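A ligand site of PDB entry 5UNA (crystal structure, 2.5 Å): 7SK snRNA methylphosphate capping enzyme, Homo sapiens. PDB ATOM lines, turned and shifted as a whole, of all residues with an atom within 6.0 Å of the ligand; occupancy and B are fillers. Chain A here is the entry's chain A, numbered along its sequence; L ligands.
A nitrogen (N1) of the ligand lies within hydrogen-bond range of the backbone carbonyl oxygen of Gly 54.
The backbone NH (N) of Ile 78 sits at hydrogen-bond distance from a nitrogen (N6) of the ligand (3.1 Å).
OD2 of Asp 77 is in hydrogen-bond range of O4 of the ligand (2.6 Å).
ND2 of Asn 56 lies within hydrogen-bond range of O4 of the ligand.
The backbone NH (N) of Tyr 163 is in hydrogen-bond range of a nitrogen (N5) of the ligand.
N4 of the ligand sits at hydrogen-bond distance from OD1 of Asn 162 (2.7 Å).
An oxygen (O1) of the ligand is in salt-bridge range of the guanidinium group (NH1) of Arg 36, at 3.0 Å.
The backbone carbonyl oxygen (O) of Leu 184 is in hydrogen-bond range of a nitrogen (N1) of the ligand.
A sulfur (S1) of the ligand sits close to the side-chain amino group of Lys 23, at 3.4 Å.
S1 of the ligand lies close to O of Gly 19 (3.8 Å).
O of Tyr 18 touches C8 of the ligand (3.3 Å).
Asn 20 touches the ligand.
Leu 53 touches the ligand (O to N1, 3.98 Å).
Leu 82 touches the ligand.
Gly 161 touches the ligand (O to C13, 3.3 Å).
Val 164 touches the ligand (CG2 to N4, 3.5 Å).
Ser 185 touches the ligand (O to C3, 3.6 Å).
CD1 of Leu 186 touches O3 of the ligand (3.3 Å).
Trp 189 touches the ligand (CD1 to C5, 3.7 Å).
Val 190 touches the ligand.
Trp 194 touches the ligand.
Hydrophobic or aromatic side chains that line the ligand: Tyr 18, Ile 78, Leu 82, Val 164, Leu 184, Leu 186, Trp 189, Val 190 and Trp 194.
21 residues have an atom within 4 Å of the ligand: Tyr 18, Gly 19, Asn 20, Lys 23, Arg 36, Leu 53, Gly 54, Asn 56, Asp 77, Ile 78, Leu 82, Gly 161, Asn 162, Tyr 163, Val 164, Leu 184, Ser 185, Leu 186, Trp 189, Val 190 and Trp 194.
The nearest printed residue that does not touch the ligand is Glu 219 (4.2 Å).
The side-chain amide nitrogen of Asn 56 lies within hydrogen-bond range of the backbone carbonyl oxygen of Tyr 21.
The backbone NH of Lys 23 lies within hydrogen-bond range of the side-chain amide oxygen of Asn 56, at 3.2 Å.
NH2 of Arg 36 is in salt-bridge range of OE1 of Glu 219.
The backbone NH of Ser 185 lies within hydrogen-bond range of the backbone carbonyl oxygen of Glu 219 (2.9 Å).
The side-chain carboxylate of Asp 77 lies within hydrogen-bond range of the backbone NH of Asn 56, at 3.0 Å.
N of Ile 78 sits close to O of Gly 161, at 3.3 Å.
OD2 of Asp 79 is in hydrogen-bond range of ND2 of Asn 20 (2.8 Å).
OD1 of Asn 20 lies within hydrogen-bond range of N of Tyr 18.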
ATOM      1  N   TYR A  18       1.407  13.663 -27.537  1.00  0.00           N
ATOM      2  CA  TYR A  18       1.584  13.799 -26.092  1.00  0.00           C
ATOM      3  C   TYR A  18       2.536  12.728 -25.591  1.00  0.00           C
ATOM      4  O   TYR A  18       2.715  12.605 -24.387  1.00  0.00           O
ATOM      5  CB  TYR A  18       0.217  13.676 -25.366  1.00  0.00           C
ATOM      6  CG  TYR A  18      -0.843  14.605 -25.917  1.00  0.00           C
ATOM      7  CD1 TYR A  18      -0.823  15.960 -25.649  1.00  0.00           C
ATOM      8  CD2 TYR A  18      -1.864  14.118 -26.728  1.00  0.00           C
ATOM      9  CE1 TYR A  18      -1.784  16.817 -26.171  1.00  0.00           C
ATOM     10  CE2 TYR A  18      -2.848  14.958 -27.232  1.00  0.00           C
ATOM     11  CZ  TYR A  18      -2.805  16.314 -26.955  1.00  0.00           C
ATOM     12  OH  TYR A  18      -3.756  17.170 -27.467  1.00  0.00           O
ATOM     13  N   GLY A  19       3.097  11.957 -26.517  1.00  0.00           N
ATOM     14  CA  GLY A  19       3.995  10.836 -26.236  1.00  0.00           C
ATOM     15  C   GLY A  19       3.151   9.673 -25.771  1.00  0.00           C
ATOM     16  O   GLY A  19       3.607   8.798 -25.047  1.00  0.00           O
ATOM     17  N   ASN A  20       1.898   9.698 -26.211  1.00  0.00           N
ATOM     18  CA  ASN A  20       0.825   8.801 -25.803  1.00  0.00           C
ATOM     19  C   ASN A  20       0.703   7.508 -26.598  1.00  0.00           C
ATOM     20  O   ASN A  20      -0.375   7.188 -27.099  1.00  0.00           O
ATOM     21  CB  ASN A  20      -0.528   9.553 -25.798  1.00  0.00           C
ATOM     22  CG  ASN A  20      -0.855  10.264 -27.082  1.00  0.00           C
ATOM     23  OD1 ASN A  20      -0.086  11.096 -27.578  1.00  0.00           O
ATOM     24  ND2 ASN A  20      -1.978   9.931 -27.639  1.00  0.00           N
ATOM     25  N   TYR A  21       1.760   6.723 -26.622  1.00  0.00           N
ATOM     26  CA  TYR A  21       1.703   5.372 -27.177  1.00  0.00           C
ATOM     27  C   TYR A  21       2.089   4.436 -26.032  1.00  0.00           C
ATOM     28  O   TYR A  21       2.641   4.903 -25.030  1.00  0.00           O
ATOM     29  CB  TYR A  21       2.546   5.172 -28.454  1.00  0.00           C
ATOM     30  CG  TYR A  21       4.028   5.378 -28.285  1.00  0.00           C
ATOM     31  CD1 TYR A  21       4.835   4.365 -27.785  1.00  0.00           C
ATOM     32  CD2 TYR A  21       4.639   6.560 -28.705  1.00  0.00           C
ATOM     33  CE1 TYR A  21       6.197   4.559 -27.607  1.00  0.00           C
ATOM     34  CE2 TYR A  21       6.008   6.749 -28.563  1.00  0.00           C
ATOM     35  CZ  TYR A  21       6.787   5.733 -28.029  1.00  0.00           C
ATOM     36  OH  TYR A  21       8.151   5.899 -27.893  1.00  0.00           O
ATOM     37  N   LYS A  23       4.033   2.317 -23.786  1.00  0.00           N
ATOM     38  CA  LYS A  23       5.420   2.215 -23.376  1.00  0.00           C
ATOM     39  C   LYS A  23       5.676   1.164 -22.307  1.00  0.00           C
ATOM     40  O   LYS A  23       5.131   1.250 -21.215  1.00  0.00           O
ATOM     41  CB  LYS A  23       5.939   3.595 -22.928  1.00  0.00           C
ATOM     42  CG  LYS A  23       6.081   4.593 -24.067  1.00  0.00           C
ATOM     43  CD  LYS A  23       6.092   6.068 -23.648  1.00  0.00           C
ATOM     44  CE  LYS A  23       6.263   6.957 -24.859  1.00  0.00           C
ATOM     45  NZ  LYS A  23       6.641   8.353 -24.541  1.00  0.00           N
ATOM     46  N   ARG A  36      13.344   1.274 -13.117  1.00  0.00           N
ATOM     47  CA  ARG A  36      13.130   2.461 -12.286  1.00  0.00           C
ATOM     48  C   ARG A  36      12.876   2.157 -10.789  1.00  0.00           C
ATOM     49  O   ARG A  36      13.171   3.012  -9.960  1.00  0.00           O
ATOM     50  CB  ARG A  36      11.980   3.300 -12.871  1.00  0.00           C
ATOM     51  CG  ARG A  36      12.438   4.212 -14.000  1.00  0.00           C
ATOM     52  CD  ARG A  36      12.115   3.644 -15.369  1.00  0.00           C
ATOM     53  NE  ARG A  36      10.676   3.530 -15.604  1.00  0.00           N
ATOM     54  CZ  ARG A  36       9.905   4.491 -16.093  1.00  0.00           C
ATOM     55  NH1 ARG A  36       8.610   4.286 -16.274  1.00  0.00           N
ATOM     56  NH2 ARG A  36      10.418   5.677 -16.410  1.00  0.00           N
ATOM     57  N   ASP A  52       0.529   9.556  -9.862  1.00  0.00           N
ATOM     58  CA  ASP A  52       1.452   9.262 -10.954  1.00  0.00           C
ATOM     59  C   ASP A  52       0.996   9.962 -12.239  1.00  0.00           C
ATOM     60  O   ASP A  52       0.063   9.510 -12.898  1.00  0.00           O
ATOM     61  CB  ASP A  52       1.627   7.733 -11.136  1.00  0.00           C
ATOM     62  CG  ASP A  52       2.588   7.296 -12.236  1.00  0.00           C
ATOM     63  OD1 ASP A  52       3.487   8.087 -12.596  1.00  0.00           O
ATOM     64  OD2 ASP A  52       2.488   6.143 -12.699  1.00  0.00           O
ATOM     65  N   LEU A  53       1.619  11.127 -12.521  1.00  0.00           N
ATOM     66  CA  LEU A  53       1.311  11.978 -13.686  1.00  0.00           C
ATOM     67  C   LEU A  53       1.811  11.358 -14.977  1.00  0.00           C
ATOM     68  O   LEU A  53       2.997  10.992 -15.055  1.00  0.00           O
ATOM     69  CB  LEU A  53       1.906  13.372 -13.491  1.00  0.00           C
ATOM     70  CG  LEU A  53       1.321  14.236 -12.396  1.00  0.00           C
ATOM     71  CD1 LEU A  53       1.931  15.620 -12.487  1.00  0.00           C
ATOM     72  CD2 LEU A  53      -0.192  14.307 -12.483  1.00  0.00           C
ATOM     73  N   GLY A  54       0.921  11.255 -15.978  1.00  0.00           N
ATOM     74  CA  GLY A  54       1.220  10.622 -17.264  1.00  0.00           C
ATOM     75  C   GLY A  54       1.600   9.164 -17.063  1.00  0.00           C
ATOM     76  O   GLY A  54       2.648   8.736 -17.507  1.00  0.00           O
ATOM     77  N   CYS A  55       0.755   8.405 -16.343  1.00  0.00           N
ATOM     78  CA  CYS A  55       0.995   7.014 -15.949  1.00  0.00           C
ATOM     79  C   CYS A  55       1.150   6.062 -17.121  1.00  0.00           C
ATOM     80  O   CYS A  55       1.692   4.979 -16.941  1.00  0.00           O
ATOM     81  CB  CYS A  55      -0.093   6.551 -14.981  1.00  0.00           C
ATOM     82  SG  CYS A  55      -1.736   6.421 -15.717  1.00  0.00           S
ATOM     83  N   ASN A  56       0.701   6.460 -18.319  1.00  0.00           N
ATOM     84  CA  ASN A  56       0.721   5.624 -19.522  1.00  0.00           C
ATOM     85  C   ASN A  56      -0.141   4.356 -19.313  1.00  0.00           C
ATOM     86  O   ASN A  56      -1.266   4.481 -18.888  1.00  0.00           O
ATOM     87  CB  ASN A  56       2.166   5.331 -20.006  1.00  0.00           C
ATOM     88  CG  ASN A  56       2.235   4.870 -21.414  1.00  0.00           C
ATOM     89  OD1 ASN A  56       2.037   3.687 -21.718  1.00  0.00           O
ATOM     90  ND2 ASN A  56       2.457   5.794 -22.319  1.00  0.00           N
ATOM     91  N   VAL A  57       0.374   3.150 -19.563  1.00  0.00           N
ATOM     92  CA  VAL A  57      -0.309   1.850 -19.382  1.00  0.00           C
ATOM     93  C   VAL A  57      -0.249   1.393 -17.928  1.00  0.00           C
ATOM     94  O   VAL A  57      -0.712   0.292 -17.600  1.00  0.00           O
ATOM     95  CB  VAL A  57       0.195   0.769 -20.381  1.00  0.00           C
ATOM     96  CG1 VAL A  57      -0.288   1.071 -21.792  1.00  0.00           C
ATOM     97  CG2 VAL A  57       1.726   0.645 -20.352  1.00  0.00           C
ATOM     98  N   LEU A  60       4.313   1.041 -13.876  1.00  0.00           N
ATOM     99  CA  LEU A  60       4.957   1.576 -12.677  1.00  0.00           C
ATOM    100  C   LEU A  60       3.962   1.816 -11.574  1.00  0.00           C
ATOM    101  O   LEU A  60       4.281   1.547 -10.411  1.00  0.00           O
ATOM    102  CB  LEU A  60       5.675   2.877 -12.983  1.00  0.00           C
ATOM    103  CG  LEU A  60       6.788   3.284 -12.033  1.00  0.00           C
ATOM    104  CD1 LEU A  60       7.836   2.156 -11.846  1.00  0.00           C
ATOM    105  CD2 LEU A  60       7.493   4.476 -12.572  1.00  0.00           C
ATOM    106  N   LEU A  76      -2.828   9.056 -13.471  1.00  0.00           N
ATOM    107  CA  LEU A  76      -3.485  10.004 -14.381  1.00  0.00           C
ATOM    108  C   LEU A  76      -2.806  10.083 -15.751  1.00  0.00           C
ATOM    109  O   LEU A  76      -1.577  10.155 -15.826  1.00  0.00           O
ATOM    110  CB  LEU A  76      -3.527  11.409 -13.743  1.00  0.00           C
ATOM    111  CG  LEU A  76      -4.091  12.531 -14.623  1.00  0.00           C
ATOM    112  CD1 LEU A  76      -5.623  12.522 -14.626  1.00  0.00           C
ATOM    113  CD2 LEU A  76      -3.572  13.868 -14.161  1.00  0.00           C
ATOM    114  N   ASP A  77      -3.602  10.102 -16.833  1.00  0.00           N
ATOM    115  CA  ASP A  77      -3.104  10.246 -18.200  1.00  0.00           C
ATOM    116  C   ASP A  77      -4.163  10.960 -19.007  1.00  0.00           C
ATOM    117  O   ASP A  77      -5.337  10.831 -18.703  1.00  0.00           O
ATOM    118  CB  ASP A  77      -2.756   8.891 -18.836  1.00  0.00           C
ATOM    119  CG  ASP A  77      -1.712   9.012 -19.956  1.00  0.00           C
ATOM    120  OD1 ASP A  77      -2.102   9.380 -21.086  1.00  0.00           O
ATOM    121  OD2 ASP A  77      -0.504   8.806 -19.682  1.00  0.00           O
ATOM    122  N   ILE A  78      -3.748  11.731 -20.019  1.00  0.00           N
ATOM    123  CA  ILE A  78      -4.609  12.483 -20.947  1.00  0.00           C
ATOM    124  C   ILE A  78      -5.377  11.536 -21.899  1.00  0.00           C
ATOM    125  O   ILE A  78      -6.515  11.826 -22.254  1.00  0.00           O
ATOM    126  CB  ILE A  78      -3.747  13.558 -21.690  1.00  0.00           C
ATOM    127  CG1 ILE A  78      -4.626  14.617 -22.396  1.00  0.00           C
ATOM    128  CG2 ILE A  78      -2.727  12.935 -22.662  1.00  0.00           C
ATOM    129  CD1 ILE A  78      -3.939  15.954 -22.614  1.00  0.00           C
ATOM    130  N   ASP A  79      -4.739  10.424 -22.294  1.00  0.00           N
ATOM    131  CA  ASP A  79      -5.228   9.410 -23.222  1.00  0.00           C
ATOM    132  C   ASP A  79      -5.995   8.268 -22.559  1.00  0.00           C
ATOM    133  O   ASP A  79      -5.421   7.448 -21.828  1.00  0.00           O
ATOM    134  CB  ASP A  79      -4.046   8.876 -24.082  1.00  0.00           C
ATOM    135  CG  ASP A  79      -4.443   8.081 -25.323  1.00  0.00           C
ATOM    136  OD1 ASP A  79      -5.504   7.426 -25.298  1.00  0.00           O
ATOM    137  OD2 ASP A  79      -3.640   8.069 -26.303  1.00  0.00           O
ATOM    138  N   LEU A  82      -4.926   4.488 -23.013  1.00  0.00           N
ATOM    139  CA  LEU A  82      -3.852   4.016 -22.131  1.00  0.00           C
ATOM    140  C   LEU A  82      -4.426   3.622 -20.786  1.00  0.00           C
ATOM    141  O   LEU A  82      -4.018   2.594 -20.269  1.00  0.00           O
ATOM    142  CB  LEU A  82      -2.712   5.049 -21.992  1.00  0.00           C
ATOM    143  CG  LEU A  82      -1.965   5.446 -23.299  1.00  0.00           C
ATOM    144  CD1 LEU A  82      -0.868   6.462 -23.049  1.00  0.00           C
ATOM    145  CD2 LEU A  82      -1.433   4.255 -24.013  1.00  0.00           C
ATOM    146  N   GLY A 161      -7.384  12.465 -17.881  1.00  0.00           N
ATOM    147  CA  GLY A 161      -7.440  13.899 -17.699  1.00  0.00           C
ATOM    148  C   GLY A 161      -6.184  14.625 -18.084  1.00  0.00           C
ATOM    149  O   GLY A 161      -5.114  14.029 -18.111  1.00  0.00           O
ATOM    150  N   ASN A 162      -6.329  15.913 -18.336  1.00  0.00           N
ATOM    151  CA  ASN A 162      -5.210  16.771 -18.636  1.00  0.00           C
ATOM    152  C   ASN A 162      -4.879  17.484 -17.327  1.00  0.00           C
ATOM    153  O   ASN A 162      -5.715  18.210 -16.796  1.00  0.00           O
ATOM    154  CB  ASN A 162      -5.584  17.773 -19.748  1.00  0.00           C
ATOM    155  CG  ASN A 162      -4.469  18.680 -20.200  1.00  0.00           C
ATOM    156  OD1 ASN A 162      -3.338  18.645 -19.721  1.00  0.00           O
ATOM    157  ND2 ASN A 162      -4.786  19.532 -21.132  1.00  0.00           N
ATOM    158  N   TYR A 163      -3.676  17.239 -16.789  1.00  0.00           N
ATOM    159  CA  TYR A 163      -3.242  17.859 -15.531  1.00  0.00           C
ATOM    160  C   TYR A 163      -3.008  19.359 -15.669  1.00  0.00           C
ATOM    161  O   TYR A 163      -3.040  20.089 -14.682  1.00  0.00           O
ATOM    162  CB  TYR A 163      -1.994  17.165 -14.990  1.00  0.00           C
ATOM    163  CG  TYR A 163      -1.779  17.404 -13.511  1.00  0.00           C
ATOM    164  CD1 TYR A 163      -2.698  16.946 -12.558  1.00  0.00           C
ATOM    165  CD2 TYR A 163      -0.682  18.122 -13.054  1.00  0.00           C
ATOM    166  CE1 TYR A 163      -2.519  17.185 -11.199  1.00  0.00           C
ATOM    167  CE2 TYR A 163      -0.473  18.357 -11.692  1.00  0.00           C
ATOM    168  CZ  TYR A 163      -1.387  17.875 -10.766  1.00  0.00           C
ATOM    169  OH  TYR A 163      -1.200  18.126  -9.439  1.00  0.00           O
ATOM    170  N   VAL A 164      -2.776  19.800 -16.910  1.00  0.00           N
ATOM    171  CA  VAL A 164      -2.543  21.215 -17.234  1.00  0.00           C
ATOM    172  C   VAL A 164      -3.850  22.001 -17.236  1.00  0.00           C
ATOM    173  O   VAL A 164      -4.727  21.768 -18.083  1.00  0.00           O
ATOM    174  CB  VAL A 164      -1.721  21.411 -18.531  1.00  0.00           C
ATOM    175  CG1 VAL A 164      -1.212  22.841 -18.633  1.00  0.00           C
ATOM    176  CG2 VAL A 164      -0.554  20.429 -18.593  1.00  0.00           C
ATOM    177  N   CYS A 183       6.392  12.613 -11.628  1.00  0.00           N
ATOM    178  CA  CYS A 183       6.360  13.348 -12.902  1.00  0.00           C
ATOM    179  C   CYS A 183       7.589  12.893 -13.684  1.00  0.00           C
ATOM    180  O   CYS A 183       8.629  13.567 -13.698  1.00  0.00           O
ATOM    181  CB  CYS A 183       6.350  14.857 -12.659  1.00  0.00           C
ATOM    182  SG  CYS A 183       6.180  15.845 -14.176  1.00  0.00           S
ATOM    183  N   LEU A 184       7.482  11.689 -14.266  1.00  0.00           N
ATOM    184  CA  LEU A 184       8.568  10.994 -14.955  1.00  0.00           C
ATOM    185  C   LEU A 184       8.364  11.005 -16.448  1.00  0.00           C
ATOM    186  O   LEU A 184       7.359  10.484 -16.910  1.00  0.00           O
ATOM    187  CB  LEU A 184       8.687   9.536 -14.433  1.00  0.00           C
ATOM    188  CG  LEU A 184       8.664   9.342 -12.910  1.00  0.00           C
ATOM    189  CD1 LEU A 184       8.462   7.890 -12.561  1.00  0.00           C
ATOM    190  CD2 LEU A 184       9.916   9.892 -12.219  1.00  0.00           C
ATOM    191  N   SER A 185       9.328  11.611 -17.211  1.00  0.00           N
ATOM    192  CA  SER A 185       9.324  11.688 -18.683  1.00  0.00           C
ATOM    193  C   SER A 185       8.079  12.402 -19.234  1.00  0.00           C
ATOM    194  O   SER A 185       7.588  12.058 -20.305  1.00  0.00           O
ATOM    195  CB  SER A 185       9.459  10.302 -19.315  1.00  0.00           C
ATOM    196  OG  SER A 185      10.605   9.603 -18.864  1.00  0.00           O
ATOM    197  N   LEU A 186       7.568  13.396 -18.491  1.00  0.00           N
ATOM    198  CA  LEU A 186       6.341  14.120 -18.851  1.00  0.00           C
ATOM    199  C   LEU A 186       6.580  15.559 -19.282  1.00  0.00           C
ATOM    200  O   LEU A 186       5.890  16.031 -20.206  1.00  0.00           O
ATOM    201  CB  LEU A 186       5.323  14.050 -17.673  1.00  0.00           C
ATOM    202  CG  LEU A 186       3.935  14.712 -17.889  1.00  0.00           C
ATOM    203  CD1 LEU A 186       3.235  14.167 -19.126  1.00  0.00           C
ATOM    204  CD2 LEU A 186       3.069  14.537 -16.702  1.00  0.00           C
ATOM    205  N   TRP A 189       6.627  16.688 -23.133  1.00  0.00           N
ATOM    206  CA  TRP A 189       5.305  16.590 -23.758  1.00  0.00           C
ATOM    207  C   TRP A 189       4.412  17.737 -23.354  1.00  0.00           C
ATOM    208  O   TRP A 189       3.735  18.306 -24.216  1.00  0.00           O
ATOM    209  CB  TRP A 189       4.690  15.216 -23.484  1.00  0.00           C
ATOM    210  CG  TRP A 189       5.556  14.094 -23.984  1.00  0.00           C
ATOM    211  CD1 TRP A 189       6.260  13.198 -23.223  1.00  0.00           C
ATOM    212  CD2 TRP A 189       5.963  13.853 -25.346  1.00  0.00           C
ATOM    213  NE1 TRP A 189       7.015  12.382 -24.021  1.00  0.00           N
ATOM    214  CE2 TRP A 189       6.844  12.754 -25.340  1.00  0.00           C
ATOM    215  CE3 TRP A 189       5.609  14.420 -26.591  1.00  0.00           C
ATOM    216  CZ2 TRP A 189       7.379  12.204 -26.513  1.00  0.00           C
ATOM    217  CZ3 TRP A 189       6.149  13.894 -27.757  1.00  0.00           C
ATOM    218  CH2 TRP A 189       7.024  12.792 -27.709  1.00  0.00           C
ATOM    219  N   VAL A 190       4.471  18.138 -22.073  1.00  0.00           N
ATOM    220  CA  VAL A 190       3.692  19.249 -21.537  1.00  0.00           C
ATOM    221  C   VAL A 190       4.224  20.583 -22.100  1.00  0.00           C
ATOM    222  O   VAL A 190       3.436  21.430 -22.511  1.00  0.00           O
ATOM    223  CB  VAL A 190       3.606  19.187 -19.994  1.00  0.00           C
ATOM    224  CG1 VAL A 190       3.088  20.490 -19.375  1.00  0.00           C
ATOM    225  CG2 VAL A 190       2.739  18.014 -19.547  1.00  0.00           C
ATOM    226  N   TRP A 194       1.847  22.704 -24.504  1.00  0.00           N
ATOM    227  CA  TRP A 194       1.257  23.841 -23.783  1.00  0.00           C
ATOM    228  C   TRP A 194       2.238  24.992 -23.410  1.00  0.00           C
ATOM    229  O   TRP A 194       1.836  25.925 -22.702  1.00  0.00           O
ATOM    230  CB  TRP A 194       0.516  23.345 -22.547  1.00  0.00           C
ATOM    231  CG  TRP A 194      -0.624  22.407 -22.865  1.00  0.00           C
ATOM    232  CD1 TRP A 194      -1.876  22.747 -23.295  1.00  0.00           C
ATOM    233  CD2 TRP A 194      -0.582  20.978 -22.837  1.00  0.00           C
ATOM    234  NE1 TRP A 194      -2.610  21.618 -23.532  1.00  0.00           N
ATOM    235  CE2 TRP A 194      -1.841  20.513 -23.270  1.00  0.00           C
ATOM    236  CE3 TRP A 194       0.395  20.033 -22.478  1.00  0.00           C
ATOM    237  CZ2 TRP A 194      -2.137  19.160 -23.383  1.00  0.00           C
ATOM    238  CZ3 TRP A 194       0.109  18.696 -22.608  1.00  0.00           C
ATOM    239  CH2 TRP A 194      -1.149  18.267 -23.048  1.00  0.00           C
ATOM    240  N   GLU A 219      11.745  13.389 -13.370  1.00  0.00           N
ATOM    241  CA  GLU A 219      12.679  12.780 -14.331  1.00  0.00           C
ATOM    242  C   GLU A 219      12.494  13.590 -15.644  1.00  0.00           C
ATOM    243  O   GLU A 219      11.675  13.222 -16.498  1.00  0.00           O
ATOM    244  CB  GLU A 219      12.389  11.274 -14.511  1.00  0.00           C
ATOM    245  CG  GLU A 219      13.403  10.512 -15.360  1.00  0.00           C
ATOM    246  CD  GLU A 219      12.874   9.340 -16.174  1.00  0.00           C
ATOM    247  OE1 GLU A 219      11.666   9.017 -16.065  1.00  0.00           O
ATOM    248  OE2 GLU A 219      13.666   8.751 -16.944  1.00  0.00           O
HETATM  249  N1  LIG L   1       5.380   8.444 -16.978  1.00  0.00           N
HETATM  250  C1  LIG L   1       5.585   7.380 -17.986  1.00  0.00           C
HETATM  251  C2  LIG L   1       5.194   7.713 -19.466  1.00  0.00           C
HETATM  252  C3  LIG L   1       5.829   8.988 -19.974  1.00  0.00           C
HETATM  253  S1  LIG L   1       5.153   9.246 -21.644  1.00  0.00           S
HETATM  254  C4  LIG L   1       7.051   6.894 -17.907  1.00  0.00           C
HETATM  255  O1  LIG L   1       7.166   5.730 -18.471  1.00  0.00           O
HETATM  256  O2  LIG L   1       7.971   7.497 -17.382  1.00  0.00           O
HETATM  257  C5  LIG L   1       4.124  10.713 -21.430  1.00  0.00           C
HETATM  258  C6  LIG L   1       2.767  10.239 -20.954  1.00  0.00           C
HETATM  259  O3  LIG L   1       2.062  11.326 -20.305  1.00  0.00           O
HETATM  260  C7  LIG L   1       1.852   9.705 -22.058  1.00  0.00           C
HETATM  261  O4  LIG L   1       1.205   8.504 -21.646  1.00  0.00           O
HETATM  262  C8  LIG L   1       0.895  10.880 -22.310  1.00  0.00           C
HETATM  263  O5  LIG L   1      -0.371  10.535 -22.866  1.00  0.00           O
HETATM  264  C9  LIG L   1       0.790  11.511 -20.911  1.00  0.00           C
HETATM  265  N2  LIG L   1       0.484  12.937 -20.879  1.00  0.00           N
HETATM  266  C10 LIG L   1       0.996  13.903 -21.712  1.00  0.00           C
HETATM  267  N3  LIG L   1       0.577  15.114 -21.442  1.00  0.00           N
HETATM  268  C11 LIG L   1      -0.279  14.939 -20.358  1.00  0.00           C
HETATM  269  C12 LIG L   1      -1.065  15.836 -19.601  1.00  0.00           C
HETATM  270  N4  LIG L   1      -1.084  17.152 -19.818  1.00  0.00           N
HETATM  271  N5  LIG L   1      -1.841  15.321 -18.618  1.00  0.00           N
HETATM  272  C13 LIG L   1      -1.822  14.005 -18.400  1.00  0.00           C
HETATM  273  N6  LIG L   1      -1.124  13.057 -19.038  1.00  0.00           N
HETATM  274  C14 LIG L   1      -0.349  13.599 -20.009  1.00  0.00           C
